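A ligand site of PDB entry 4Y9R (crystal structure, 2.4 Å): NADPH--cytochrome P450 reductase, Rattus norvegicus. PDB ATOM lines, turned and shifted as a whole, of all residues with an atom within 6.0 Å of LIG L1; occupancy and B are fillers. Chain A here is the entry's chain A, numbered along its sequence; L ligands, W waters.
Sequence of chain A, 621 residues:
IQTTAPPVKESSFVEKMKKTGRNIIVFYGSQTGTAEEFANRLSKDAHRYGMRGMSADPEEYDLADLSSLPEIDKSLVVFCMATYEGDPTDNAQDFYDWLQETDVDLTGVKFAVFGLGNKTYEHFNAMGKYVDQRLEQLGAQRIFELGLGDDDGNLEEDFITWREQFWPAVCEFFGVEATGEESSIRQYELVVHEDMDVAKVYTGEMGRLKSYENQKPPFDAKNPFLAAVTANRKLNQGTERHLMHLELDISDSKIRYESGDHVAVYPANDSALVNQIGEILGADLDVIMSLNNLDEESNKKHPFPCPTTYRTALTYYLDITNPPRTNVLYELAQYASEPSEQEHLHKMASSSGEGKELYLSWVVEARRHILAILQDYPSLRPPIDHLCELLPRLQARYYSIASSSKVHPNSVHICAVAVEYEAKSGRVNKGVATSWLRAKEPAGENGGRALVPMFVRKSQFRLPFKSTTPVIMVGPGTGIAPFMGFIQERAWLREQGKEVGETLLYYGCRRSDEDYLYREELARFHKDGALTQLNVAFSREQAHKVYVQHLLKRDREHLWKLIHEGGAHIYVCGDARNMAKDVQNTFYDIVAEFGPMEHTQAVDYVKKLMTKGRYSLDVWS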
ATOM      1  N   GLY A  29     -11.781  25.343 -17.707  1.00  0.00           N
ATOM      2  CA  GLY A  29     -12.241  24.873 -16.430  1.00  0.00           C
ATOM      3  C   GLY A  29     -11.161  25.263 -15.462  1.00  0.00           C
ATOM      4  O   GLY A  29     -10.097  24.644 -15.413  1.00  0.00           O
ATOM      5  N   SER A  30     -11.423  26.314 -14.683  1.00  0.00           N
ATOM      6  CA  SER A  30     -10.417  26.863 -13.798  1.00  0.00           C
ATOM      7  C   SER A  30     -11.043  27.271 -12.478  1.00  0.00           C
ATOM      8  O   SER A  30     -12.236  27.548 -12.406  1.00  0.00           O
ATOM      9  CB  SER A  30      -9.734  28.074 -14.444  1.00  0.00           C
ATOM     10  OG  SER A  30      -8.600  28.474 -13.708  1.00  0.00           O
ATOM     11  N   GLN A  31     -10.228  27.291 -11.438  1.00  0.00           N
ATOM     12  CA  GLN A  31     -10.724  27.657 -10.120  1.00  0.00           C
ATOM     13  C   GLN A  31      -9.791  28.692  -9.508  1.00  0.00           C
ATOM     14  O   GLN A  31     -10.211  29.517  -8.704  1.00  0.00           O
ATOM     15  CB  GLN A  31     -10.806  26.415  -9.235  1.00  0.00           C
ATOM     16  CG  GLN A  31     -11.880  26.490  -8.187  1.00  0.00           C
ATOM     17  CD  GLN A  31     -12.255  25.124  -7.636  1.00  0.00           C
ATOM     18  OE1 GLN A  31     -12.723  24.253  -8.383  1.00  0.00           O
ATOM     19  NE2 GLN A  31     -12.037  24.923  -6.341  1.00  0.00           N
ATOM     20  N   THR A  32      -8.525  28.652  -9.930  1.00  0.00           N
ATOM     21  CA  THR A  32      -7.502  29.576  -9.449  1.00  0.00           C
ATOM     22  C   THR A  32      -6.957  30.428 -10.587  1.00  0.00           C
ATOM     23  O   THR A  32      -5.928  31.107 -10.463  1.00  0.00           O
ATOM     24  CB  THR A  32      -6.346  28.804  -8.768  1.00  0.00           C
ATOM     25  OG1 THR A  32      -6.875  27.981  -7.721  1.00  0.00           O
ATOM     26  CG2 THR A  32      -5.327  29.761  -8.201  1.00  0.00           C
ATOM     27  N   GLY A  33      -7.646  30.385 -11.729  1.00  0.00           N
ATOM     28  CA  GLY A  33      -7.233  31.175 -12.879  1.00  0.00           C
ATOM     29  C   GLY A  33      -6.080  30.655 -13.719  1.00  0.00           C
ATOM     30  O   GLY A  33      -5.578  31.388 -14.561  1.00  0.00           O
ATOM     31  N   THR A  34      -5.646  29.416 -13.500  1.00  0.00           N
ATOM     32  CA  THR A  34      -4.534  28.876 -14.283  1.00  0.00           C
ATOM     33  C   THR A  34      -5.003  28.468 -15.681  1.00  0.00           C
ATOM     34  O   THR A  34      -4.481  28.943 -16.684  1.00  0.00           O
ATOM     35  CB  THR A  34      -3.916  27.639 -13.612  1.00  0.00           C
ATOM     36  OG1 THR A  34      -3.588  27.933 -12.252  1.00  0.00           O
ATOM     37  CG2 THR A  34      -2.637  27.239 -14.345  1.00  0.00           C
ATOM     38  N   ALA A  35      -5.990  27.582 -15.730  1.00  0.00           N
ATOM     39  CA  ALA A  35      -6.558  27.105 -16.983  1.00  0.00           C
ATOM     40  C   ALA A  35      -7.151  28.287 -17.735  1.00  0.00           C
ATOM     41  O   ALA A  35      -7.185  28.303 -18.963  1.00  0.00           O
ATOM     42  CB  ALA A  35      -7.647  26.067 -16.709  1.00  0.00           C
ATOM     43  N   GLU A  36      -7.605  29.296 -17.003  1.00  0.00           N
ATOM     44  CA  GLU A  36      -8.165  30.454 -17.661  1.00  0.00           C
ATOM     45  C   GLU A  36      -7.075  31.220 -18.420  1.00  0.00           C
ATOM     46  O   GLU A  36      -7.332  31.770 -19.484  1.00  0.00           O
ATOM     47  CB  GLU A  36      -8.868  31.371 -16.642  1.00  0.00           C
ATOM     48  CG  GLU A  36      -9.221  32.738 -17.183  1.00  0.00           C
ATOM     49  CD  GLU A  36     -10.247  33.459 -16.330  1.00  0.00           C
ATOM     50  OE1 GLU A  36     -10.223  33.262 -15.089  1.00  0.00           O
ATOM     51  OE2 GLU A  36     -11.066  34.219 -16.895  1.00  0.00           O
ATOM     52  N   ALA A  82      -8.885  21.952 -15.502  1.00  0.00           N
ATOM     53  CA  ALA A  82      -8.152  21.586 -14.291  1.00  0.00           C
ATOM     54  C   ALA A  82      -9.029  20.649 -13.470  1.00  0.00           C
ATOM     55  O   ALA A  82     -10.254  20.622 -13.644  1.00  0.00           O
ATOM     56  CB  ALA A  82      -7.819  22.833 -13.480  1.00  0.00           C
ATOM     57  N   THR A  83      -8.408  19.878 -12.594  1.00  0.00           N
ATOM     58  CA  THR A  83      -9.137  18.940 -11.753  1.00  0.00           C
ATOM     59  C   THR A  83      -9.075  19.315 -10.278  1.00  0.00           C
ATOM     60  O   THR A  83      -8.087  19.879  -9.810  1.00  0.00           O
ATOM     61  CB  THR A  83      -8.577  17.507 -11.896  1.00  0.00           C
ATOM     62  OG1 THR A  83      -8.853  17.024 -13.215  1.00  0.00           O
ATOM     63  CG2 THR A  83      -9.200  16.589 -10.869  1.00  0.00           C
ATOM     64  N   TYR A  84     -10.143  19.018  -9.547  1.00  0.00           N
ATOM     65  CA  TYR A  84     -10.164  19.303  -8.119  1.00  0.00           C
ATOM     66  C   TYR A  84     -10.790  18.151  -7.360  1.00  0.00           C
ATOM     67  O   TYR A  84     -12.002  17.944  -7.408  1.00  0.00           O
ATOM     68  CB  TYR A  84     -10.906  20.601  -7.834  1.00  0.00           C
ATOM     69  CG  TYR A  84     -10.040  21.820  -8.020  1.00  0.00           C
ATOM     70  CD1 TYR A  84      -9.628  22.236  -9.291  1.00  0.00           C
ATOM     71  CD2 TYR A  84      -9.592  22.554  -6.924  1.00  0.00           C
ATOM     72  CE1 TYR A  84      -8.795  23.338  -9.461  1.00  0.00           C
ATOM     73  CE2 TYR A  84      -8.768  23.662  -7.075  1.00  0.00           C
ATOM     74  CZ  TYR A  84      -8.361  24.048  -8.351  1.00  0.00           C
ATOM     75  OH  TYR A  84      -7.547  25.144  -8.482  1.00  0.00           O
ATOM     76  N   GLU A  85      -9.936  17.396  -6.671  1.00  0.00           N
ATOM     77  CA  GLU A  85     -10.344  16.240  -5.891  1.00  0.00           C
ATOM     78  C   GLU A  85     -11.090  15.245  -6.786  1.00  0.00           C
ATOM     79  O   GLU A  85     -12.123  14.705  -6.408  1.00  0.00           O
ATOM     80  CB  GLU A  85     -11.225  16.663  -4.714  1.00  0.00           C
ATOM     81  CG  GLU A  85     -10.491  17.466  -3.651  1.00  0.00           C
ATOM     82  CD  GLU A  85      -9.173  16.813  -3.250  1.00  0.00           C
ATOM     83  OE1 GLU A  85      -9.151  15.597  -2.982  1.00  0.00           O
ATOM     84  OE2 GLU A  85      -8.150  17.533  -3.216  1.00  0.00           O
ATOM     85  N   GLY A  86     -10.549  15.023  -7.978  1.00  0.00           N
ATOM     86  CA  GLY A  86     -11.150  14.097  -8.913  1.00  0.00           C
ATOM     87  C   GLY A  86     -12.415  14.639  -9.560  1.00  0.00           C
ATOM     88  O   GLY A  86     -13.023  13.972 -10.393  1.00  0.00           O
ATOM     89  N   ASP A  87     -12.801  15.857  -9.182  1.00  0.00           N
ATOM     90  CA  ASP A  87     -13.995  16.499  -9.730  1.00  0.00           C
ATOM     91  C   ASP A  87     -13.656  17.614 -10.711  1.00  0.00           C
ATOM     92  O   ASP A  87     -12.505  18.040 -10.823  1.00  0.00           O
ATOM     93  CB  ASP A  87     -14.841  17.126  -8.616  1.00  0.00           C
ATOM     94  CG  ASP A  87     -15.391  16.113  -7.636  1.00  0.00           C
ATOM     95  OD1 ASP A  87     -16.134  15.193  -8.069  1.00  0.00           O
ATOM     96  OD2 ASP A  87     -15.089  16.239  -6.433  1.00  0.00           O
ATOM     97  N   THR A  89     -13.928  21.541 -12.106  1.00  0.00           N
ATOM     98  CA  THR A  89     -13.944  22.793 -11.359  1.00  0.00           C
ATOM     99  C   THR A  89     -15.408  23.192 -11.200  1.00  0.00           C
ATOM    100  O   THR A  89     -16.272  22.629 -11.884  1.00  0.00           O
ATOM    101  CB  THR A  89     -13.169  23.910 -12.098  1.00  0.00           C
ATOM    102  OG1 THR A  89     -13.688  24.060 -13.424  1.00  0.00           O
ATOM    103  CG2 THR A  89     -11.688  23.551 -12.172  1.00  0.00           C
ATOM    104  N   LEU A 116      -5.043  20.289 -16.575  1.00  0.00           N
ATOM    105  CA  LEU A 116      -4.176  20.825 -15.530  1.00  0.00           C
ATOM    106  C   LEU A 116      -4.355  19.968 -14.289  1.00  0.00           C
ATOM    107  O   LEU A 116      -5.357  20.090 -13.582  1.00  0.00           O
ATOM    108  CB  LEU A 116      -4.552  22.275 -15.190  1.00  0.00           C
ATOM    109  CG  LEU A 116      -4.221  23.401 -16.168  1.00  0.00           C
ATOM    110  CD1 LEU A 116      -4.957  23.225 -17.481  1.00  0.00           C
ATOM    111  CD2 LEU A 116      -4.583  24.716 -15.524  1.00  0.00           C
ATOM    112  N   GLY A 117      -3.402  19.071 -14.052  1.00  0.00           N
ATOM    113  CA  GLY A 117      -3.496  18.132 -12.962  1.00  0.00           C
ATOM    114  C   GLY A 117      -2.308  18.208 -12.031  1.00  0.00           C
ATOM    115  O   GLY A 117      -1.449  19.086 -12.165  1.00  0.00           O
ATOM    116  N   ASN A 118      -2.252  17.276 -11.085  1.00  0.00           N
ATOM    117  CA  ASN A 118      -1.119  17.183 -10.167  1.00  0.00           C
ATOM    118  C   ASN A 118      -1.043  15.681  -9.914  1.00  0.00           C
ATOM    119  O   ASN A 118      -2.016  15.068  -9.476  1.00  0.00           O
ATOM    120  CB  ASN A 118      -1.168  17.942  -8.839  1.00  0.00           C
ATOM    121  CG  ASN A 118       0.138  17.827  -8.066  1.00  0.00           C
ATOM    122  OD1 ASN A 118       0.816  16.808  -8.124  1.00  0.00           O
ATOM    123  ND2 ASN A 118       0.472  18.884  -7.332  1.00  0.00           N
ATOM    124  N   LYS A 119       0.135  15.139 -10.209  1.00  0.00           N
ATOM    125  CA  LYS A 119       0.436  13.717 -10.138  1.00  0.00           C
ATOM    126  C   LYS A 119       0.306  13.166  -8.735  1.00  0.00           C
ATOM    127  O   LYS A 119      -0.137  12.038  -8.542  1.00  0.00           O
ATOM    128  CB  LYS A 119       1.839  13.447 -10.688  1.00  0.00           C
ATOM    129  CG  LYS A 119       1.906  13.355 -12.206  1.00  0.00           C
ATOM    130  CD  LYS A 119       2.775  12.196 -12.656  1.00  0.00           C
ATOM    131  CE  LYS A 119       3.388  12.470 -14.021  1.00  0.00           C
ATOM    132  NZ  LYS A 119       3.637  13.915 -14.239  1.00  0.00           N
ATOM    133  N   TYR A 121      -1.652  12.932  -6.689  1.00  0.00           N
ATOM    134  CA  TYR A 121      -3.062  12.801  -6.389  1.00  0.00           C
ATOM    135  C   TYR A 121      -3.500  11.455  -6.938  1.00  0.00           C
ATOM    136  O   TYR A 121      -2.898  10.933  -7.876  1.00  0.00           O
ATOM    137  CB  TYR A 121      -3.865  13.927  -7.033  1.00  0.00           C
ATOM    138  CG  TYR A 121      -3.820  15.227  -6.274  1.00  0.00           C
ATOM    139  CD1 TYR A 121      -2.699  16.038  -6.314  1.00  0.00           C
ATOM    140  CD2 TYR A 121      -4.896  15.646  -5.513  1.00  0.00           C
ATOM    141  CE1 TYR A 121      -2.649  17.229  -5.625  1.00  0.00           C
ATOM    142  CE2 TYR A 121      -4.855  16.836  -4.813  1.00  0.00           C
ATOM    143  CZ  TYR A 121      -3.723  17.625  -4.873  1.00  0.00           C
ATOM    144  OH  TYR A 121      -3.682  18.816  -4.173  1.00  0.00           O
ATOM    145  N   HIS A 123      -6.501  10.893  -8.308  1.00  0.00           N
ATOM    146  CA  HIS A 123      -7.179  11.244  -9.550  1.00  0.00           C
ATOM    147  C   HIS A 123      -6.485  12.427 -10.223  1.00  0.00           C
ATOM    148  O   HIS A 123      -6.868  13.589 -10.040  1.00  0.00           O
ATOM    149  CB  HIS A 123      -8.648  11.561  -9.249  1.00  0.00           C
ATOM    150  CG  HIS A 123      -9.365  10.435  -8.581  1.00  0.00           C
ATOM    151  ND1 HIS A 123      -9.464   9.177  -9.132  1.00  0.00           N
ATOM    152  CD2 HIS A 123     -10.016  10.375  -7.393  1.00  0.00           C
ATOM    153  CE1 HIS A 123     -10.146   8.386  -8.312  1.00  0.00           C
ATOM    154  NE2 HIS A 123     -10.490   9.090  -7.255  1.00  0.00           N
ATOM    155  N   PHE A 124      -5.472  12.098 -11.019  1.00  0.00           N
ATOM    156  CA  PHE A 124      -4.656  13.055 -11.752  1.00  0.00           C
ATOM    157  C   PHE A 124      -5.225  13.383 -13.133  1.00  0.00           C
ATOM    158  O   PHE A 124      -5.325  12.509 -13.987  1.00  0.00           O
ATOM    159  CB  PHE A 124      -3.245  12.480 -11.894  1.00  0.00           C
ATOM    160  CG  PHE A 124      -2.373  13.216 -12.858  1.00  0.00           C
ATOM    161  CD1 PHE A 124      -1.985  14.523 -12.620  1.00  0.00           C
ATOM    162  CD2 PHE A 124      -1.922  12.581 -14.009  1.00  0.00           C
ATOM    163  CE1 PHE A 124      -1.157  15.193 -13.495  1.00  0.00           C
ATOM    164  CE2 PHE A 124      -1.091  13.240 -14.901  1.00  0.00           C
ATOM    165  CZ  PHE A 124      -0.705  14.557 -14.645  1.00  0.00           C
ATOM    166  N   ASN A 125      -5.589  14.642 -13.345  1.00  0.00           N
ATOM    167  CA  ASN A 125      -6.145  15.073 -14.625  1.00  0.00           C
ATOM    168  C   ASN A 125      -7.383  14.261 -15.005  1.00  0.00           C
ATOM    169  O   ASN A 125      -7.604  13.959 -16.172  1.00  0.00           O
ATOM    170  CB  ASN A 125      -5.097  14.933 -15.730  1.00  0.00           C
ATOM    171  CG  ASN A 125      -4.235  16.187 -15.891  1.00  0.00           C
ATOM    172  OD1 ASN A 125      -4.634  17.271 -15.485  1.00  0.00           O
ATOM    173  ND2 ASN A 125      -3.046  16.024 -16.471  1.00  0.00           N
ATOM    174  N   ALA A 126      -8.201  13.920 -14.013  1.00  0.00           N
ATOM    175  CA  ALA A 126      -9.418  13.137 -14.263  1.00  0.00           C
ATOM    176  C   ALA A 126     -10.363  13.844 -15.213  1.00  0.00           C
ATOM    177  O   ALA A 126     -10.890  13.239 -16.151  1.00  0.00           O
ATOM    178  CB  ALA A 126     -10.118  12.842 -12.944  1.00  0.00           C
ATOM    179  N   ASP A 151       1.286  19.947 -12.201  1.00  0.00           N
ATOM    180  CA  ASP A 151       1.706  21.070 -11.365  1.00  0.00           C
ATOM    181  C   ASP A 151       2.724  20.601 -10.326  1.00  0.00           C
ATOM    182  O   ASP A 151       3.195  21.390  -9.510  1.00  0.00           O
ATOM    183  CB  ASP A 151       0.468  21.686 -10.689  1.00  0.00           C
ATOM    184  CG  ASP A 151       0.728  23.095 -10.172  1.00  0.00           C
ATOM    185  OD1 ASP A 151       1.177  23.952 -10.960  1.00  0.00           O
ATOM    186  OD2 ASP A 151       0.450  23.349  -8.979  1.00  0.00           O
ATOM    187  N   LEU A 155       3.962  22.904 -14.562  1.00  0.00           N
ATOM    188  CA  LEU A 155       2.814  22.979 -15.458  1.00  0.00           C
ATOM    189  C   LEU A 155       3.037  23.930 -16.611  1.00  0.00           C
ATOM    190  O   LEU A 155       2.692  23.622 -17.755  1.00  0.00           O
ATOM    191  CB  LEU A 155       1.571  23.386 -14.662  1.00  0.00           C
ATOM    192  CG  LEU A 155       0.241  23.435 -15.394  1.00  0.00           C
ATOM    193  CD1 LEU A 155       0.015  22.164 -16.197  1.00  0.00           C
ATOM    194  CD2 LEU A 155      -0.863  23.632 -14.372  1.00  0.00           C
ATOM    195  N   ARG A 457     -16.820  28.664   1.683  1.00  0.00           N
ATOM    196  CA  ARG A 457     -16.955  27.693   0.598  1.00  0.00           C
ATOM    197  C   ARG A 457     -17.202  26.371   1.270  1.00  0.00           C
ATOM    198  O   ARG A 457     -16.407  25.914   2.075  1.00  0.00           O
ATOM    199  CB  ARG A 457     -15.681  27.600  -0.251  1.00  0.00           C
ATOM    200  CG  ARG A 457     -15.868  26.663  -1.453  1.00  0.00           C
ATOM    201  CD  ARG A 457     -14.596  26.465  -2.254  1.00  0.00           C
ATOM    202  NE  ARG A 457     -13.592  25.716  -1.500  1.00  0.00           N
ATOM    203  CZ  ARG A 457     -12.310  25.612  -1.851  1.00  0.00           C
ATOM    204  NH1 ARG A 457     -11.873  26.218  -2.956  1.00  0.00           N
ATOM    205  NH2 ARG A 457     -11.465  24.920  -1.097  1.00  0.00           N
ATOM    206  N   VAL A 619      -5.925  18.574   2.697  1.00  0.00           N
ATOM    207  CA  VAL A 619      -4.501  18.837   2.613  1.00  0.00           C
ATOM    208  C   VAL A 619      -4.203  19.847   1.527  1.00  0.00           C
ATOM    209  O   VAL A 619      -5.030  20.085   0.637  1.00  0.00           O
ATOM    210  CB  VAL A 619      -3.748  17.528   2.362  1.00  0.00           C
ATOM    211  CG1 VAL A 619      -3.998  16.571   3.503  1.00  0.00           C
ATOM    212  CG2 VAL A 619      -4.234  16.893   1.058  1.00  0.00           C
HETATM  213  N1  LIG L   1      -4.894  17.951  -9.456  1.00  0.00           N
HETATM  214  C1  LIG L   1      -5.292  16.733  -9.892  1.00  0.00           C
HETATM  215  O1  LIG L   1      -4.775  16.196 -10.894  1.00  0.00           O
HETATM  216  N2  LIG L   1      -6.284  16.116  -9.162  1.00  0.00           N
HETATM  217  C2  LIG L   1      -6.928  16.600  -8.019  1.00  0.00           C
HETATM  218  O2  LIG L   1      -7.780  15.858  -7.549  1.00  0.00           O
HETATM  219  C3  LIG L   1      -6.521  17.870  -7.556  1.00  0.00           C
HETATM  220  N3  LIG L   1      -7.162  18.377  -6.392  1.00  0.00           N
HETATM  221  C4  LIG L   1      -6.704  19.644  -6.007  1.00  0.00           C
HETATM  222  C5  LIG L   1      -7.333  20.180  -4.824  1.00  0.00           C
HETATM  223  C6  LIG L   1      -6.968  21.460  -4.313  1.00  0.00           C
HETATM  224  C7  LIG L   1      -7.732  21.909  -3.040  1.00  0.00           C
HETATM  225  C8  LIG L   1      -5.904  22.282  -4.992  1.00  0.00           C
HETATM  226  C9  LIG L   1      -5.468  23.536  -4.588  1.00  0.00           C
HETATM  227  C10 LIG L   1      -5.294  21.762  -6.127  1.00  0.00           C
HETATM  228  C11 LIG L   1      -5.661  20.448  -6.676  1.00  0.00           C
HETATM  229  N4  LIG L   1      -5.055  19.830  -7.878  1.00  0.00           N
HETATM  230  C12 LIG L   1      -5.490  18.501  -8.328  1.00  0.00           C
HETATM  231  C13 LIG L   1      -4.025  20.552  -8.603  1.00  0.00           C
HETATM  232  C14 LIG L   1      -4.626  21.477  -9.704  1.00  0.00           C
HETATM  233  O3  LIG L   1      -5.339  20.610 -10.684  1.00  0.00           O
HETATM  234  C15 LIG L   1      -3.549  22.265 -10.419  1.00  0.00           C
HETATM  235  O4  LIG L   1      -2.902  23.088  -9.419  1.00  0.00           O
HETATM  236  C16 LIG L   1      -4.227  23.163 -11.525  1.00  0.00           C
HETATM  237  O5  LIG L   1      -3.073  23.802 -12.127  1.00  0.00           O
HETATM  238  C17 LIG L   1      -5.108  24.279 -10.963  1.00  0.00           C
HETATM  239  O6  LIG L   1      -5.744  25.098 -12.032  1.00  0.00           O
HETATM  240  P1  LIG L   1      -6.688  26.343 -11.836  1.00  0.00           P
HETATM  241  O7  LIG L   1      -5.926  27.481 -11.258  1.00  0.00           O
HETATM  242  O8  LIG L   1      -7.926  25.768 -11.083  1.00  0.00           O
HETATM  243  O9  LIG L   1      -7.014  26.699 -13.363  1.00  0.00           O
HETATM  244  P1  LG2 L   2       1.538  33.305  -1.007  1.00  0.00           P
HETATM  245  O1  LG2 L   2       1.926  34.693  -1.362  1.00  0.00           O
HETATM  246  O2  LG2 L   2       0.317  32.722  -1.603  1.00  0.00           O
HETATM  247  O3  LG2 L   2       2.790  32.345  -1.308  1.00  0.00           O
HETATM  248  C1  LG2 L   2       2.623  30.923  -1.327  1.00  0.00           C
HETATM  249  C2  LG2 L   2       3.792  30.282  -2.080  1.00  0.00           C
HETATM  250  O4  LG2 L   2       5.052  30.635  -1.491  1.00  0.00           O
HETATM  251  C3  LG2 L   2       3.787  28.778  -1.922  1.00  0.00           C
HETATM  252  O5  LG2 L   2       2.802  28.212  -2.792  1.00  0.00           O
HETATM  253  C4  LG2 L   2       5.169  28.471  -2.462  1.00  0.00           C
HETATM  254  O6  LG2 L   2       5.145  28.468  -3.895  1.00  0.00           O
HETATM  255  C5  LG2 L   2       5.994  29.647  -1.950  1.00  0.00           C
HETATM  256  N1  LG2 L   2       6.825  29.268  -0.791  1.00  0.00           N
HETATM  257  C6  LG2 L   2       6.367  29.139   0.606  1.00  0.00           C
HETATM  258  N2  LG2 L   2       7.653  28.868   1.288  1.00  0.00           N
HETATM  259  C7  LG2 L   2       8.614  28.770   0.375  1.00  0.00           C
HETATM  260  C8  LG2 L   2       9.907  28.528   0.537  1.00  0.00           C
HETATM  261  N3  LG2 L   2      10.319  28.375   1.801  1.00  0.00           N
HETATM  262  N4  LG2 L   2      10.773  28.450  -0.489  1.00  0.00           N
HETATM  263  C9  LG2 L   2      10.285  28.630  -1.782  1.00  0.00           C
HETATM  264  N5  LG2 L   2       8.911  28.874  -1.931  1.00  0.00           N
HETATM  265  C10 LG2 L   2       8.118  28.943  -0.852  1.00  0.00           C
HETATM  266  N6  LG2 L   2      -2.793  27.500   5.361  1.00  0.00           N
HETATM  267  C11 LG2 L   2      -2.813  27.653   6.757  1.00  0.00           C
HETATM  268  O7  LG2 L   2      -1.835  28.112   7.346  1.00  0.00           O
HETATM  269  N7  LG2 L   2      -3.909  27.188   7.479  1.00  0.00           N
HETATM  270  C12 LG2 L   2      -4.973  26.565   6.821  1.00  0.00           C
HETATM  271  O8  LG2 L   2      -5.973  26.226   7.468  1.00  0.00           O
HETATM  272  C13 LG2 L   2      -4.941  26.407   5.442  1.00  0.00           C
HETATM  273  N8  LG2 L   2      -5.878  25.661   4.838  1.00  0.00           N
HETATM  274  C14 LG2 L   2      -5.850  25.514   3.499  1.00  0.00           C
HETATM  275  C15 LG2 L   2      -6.887  24.840   2.868  1.00  0.00           C
HETATM  276  C16 LG2 L   2      -6.942  24.794   1.473  1.00  0.00           C
HETATM  277  C17 LG2 L   2      -8.071  24.255   0.858  1.00  0.00           C
HETATM  278  C18 LG2 L   2      -5.955  25.405   0.721  1.00  0.00           C
HETATM  279  C19 LG2 L   2      -5.974  25.320  -0.667  1.00  0.00           C
HETATM  280  C20 LG2 L   2      -4.913  26.080   1.365  1.00  0.00           C
HETATM  281  C21 LG2 L   2      -4.864  26.143   2.748  1.00  0.00           C
HETATM  282  N9  LG2 L   2      -3.899  26.849   3.371  1.00  0.00           N
HETATM  283  C22 LG2 L   2      -3.851  26.860   4.716  1.00  0.00           C
HETATM  284  C23 LG2 L   2      -2.841  27.532   2.603  1.00  0.00           C
HETATM  285  C24 LG2 L   2      -3.289  28.952   2.257  1.00  0.00           C
HETATM  286  O9  LG2 L   2      -4.387  28.891   1.341  1.00  0.00           O
HETATM  287  C25 LG2 L   2      -2.160  29.775   1.635  1.00  0.00           C
HETATM  288  O10 LG2 L   2      -1.595  29.086   0.513  1.00  0.00           O
HETATM  289  C26 LG2 L   2      -1.070  30.049   2.685  1.00  0.00           C
HETATM  290  O11 LG2 L   2      -1.634  30.721   3.807  1.00  0.00           O
HETATM  291  C27 LG2 L   2      -0.005  30.951   2.037  1.00  0.00           C
HETATM  292  O12 LG2 L   2      -0.664  32.042   1.399  1.00  0.00           O
HETATM  293  P2  LG2 L   2       0.008  33.506   1.335  1.00  0.00           P
HETATM  294  O13 LG2 L   2       0.306  33.960   2.715  1.00  0.00           O
HETATM  295  O14 LG2 L   2      -0.839  34.361   0.481  1.00  0.00           O
HETATM  296  O15 LG2 L   2       1.412  33.215   0.592  1.00  0.00           O
HETATM  297  O   HOH W   1      -3.763  25.553  -7.314  1.00  0.00           O
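Ala 82 touches LIG L1 (CB to O6, 3.4 Å).
CA of Gly 117 touches O1 of LIG L1 (3.1 Å).
CE2 of Tyr 121 touches N3 of LIG L1 (3.2 Å).
CA of Phe 124 touches O1 of LIG L1, at 3.3 Å.
Leu 155 touches LIG L1 (CD2 to O5, 3.2 Å).
Hydrophobic or aromatic side chains that line LIG L1: Ala 35, Ala 82, Tyr 84, Leu 116, Tyr 121, Phe 124 and Leu 155.
20 residues have an atom within 4 Å of LIG L1: Ser 30, Gln 31, Thr 32, Gly 33, Thr 34, Ala 35, Ala 82, Thr 83, Tyr 84, Glu 85, Gly 86, Leu 116, Gly 117, Asn 118, Tyr 121, His 123, Phe 124, Asn 125, Asp 151 and Leu 155.
The nearest printed residue that does not touch LIG L1 is Gly 29 (4.2 Å).
OG of Ser 30 sits at hydrogen-bond distance from O9 of LIG L1, at 2.4 Å.
The backbone NH of Thr 34 sits at hydrogen-bond distance from an oxygen (O7) of LIG L1 (3.0 Å).
OG1 of Thr 34 sits at hydrogen-bond distance from O7 of LIG L1, 2.6 Å away.
An oxygen (O8) of LIG L1 is in hydrogen-bond range of the side-chain hydroxyl (OH) of Tyr 84.
An oxygen (O9) of LIG L1 sits at hydrogen-bond distance from the backbone NH of Ala 35 (2.7 Å).
O of His 123 is in hydrogen-bond range of N2 of LIG L1 (2.7 Å).
An oxygen (O1) of LIG L1 sits at hydrogen-bond distance from the backbone NH (N) of Asn 118 (2.8 Å).
An oxygen (O8) of LIG L1 is in hydrogen-bond range of the backbone NH of Gln 31 (2.8 Å).
The backbone NH (N) of Glu 85 sits at hydrogen-bond distance from an oxygen (O2) of LIG L1, 2.8 Å away.
N of Thr 32 sits close to O7 of LIG L1, at 3.1 Å.
The backbone NH (N) of Gly 86 sits at hydrogen-bond distance from an oxygen (O2) of LIG L1 (2.9 Å).
The backbone carbonyl oxygen (O) of Leu 116 is in hydrogen-bond range of an oxygen (O3) of LIG L1 (2.9 Å).
O of Thr 83 is in hydrogen-bond range of O3 of LIG L1 (3.0 Å).
The backbone NH (N) of Asn 125 sits at hydrogen-bond distance from an oxygen (O1) of LIG L1, at 3.0 Å.
The side-chain carboxylate of Asp 151 sits at hydrogen-bond distance from an oxygen (O4) of LIG L1.
O7 of LIG L1 lies within hydrogen-bond range of N of Gly 33 (3.4 Å).
The side-chain hydroxyl (OG) of Ser 30 lies within hydrogen-bond range of the backbone NH (N) of Thr 34, 3.1 Å away.
The backbone NH (N) of Ala 35 sits at hydrogen-bond distance from the side-chain hydroxyl (OG) of Ser 30, at 3.4 Å.
The side-chain hydroxyl of Thr 89 lies within hydrogen-bond range of the backbone NH of Ser 30.
OG1 of Thr 32 is in hydrogen-bond range of OH of Tyr 84, 3.0 Å away.
The backbone carbonyl oxygen (O) of Leu 116 sits at hydrogen-bond distance from the backbone NH (N) of Thr 83.
The side-chain amide oxygen (OD1) of Asn 125 lies close to the backbone NH (N) of Leu 116 (3.2 Å).
The backbone NH (N) of Asp 151 lies within hydrogen-bond range of the backbone carbonyl oxygen (O) of Gly 117 (2.9 Å).
O of Gly 29 is in hydrogen-bond range of N of Ala 82 (3.0 Å).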
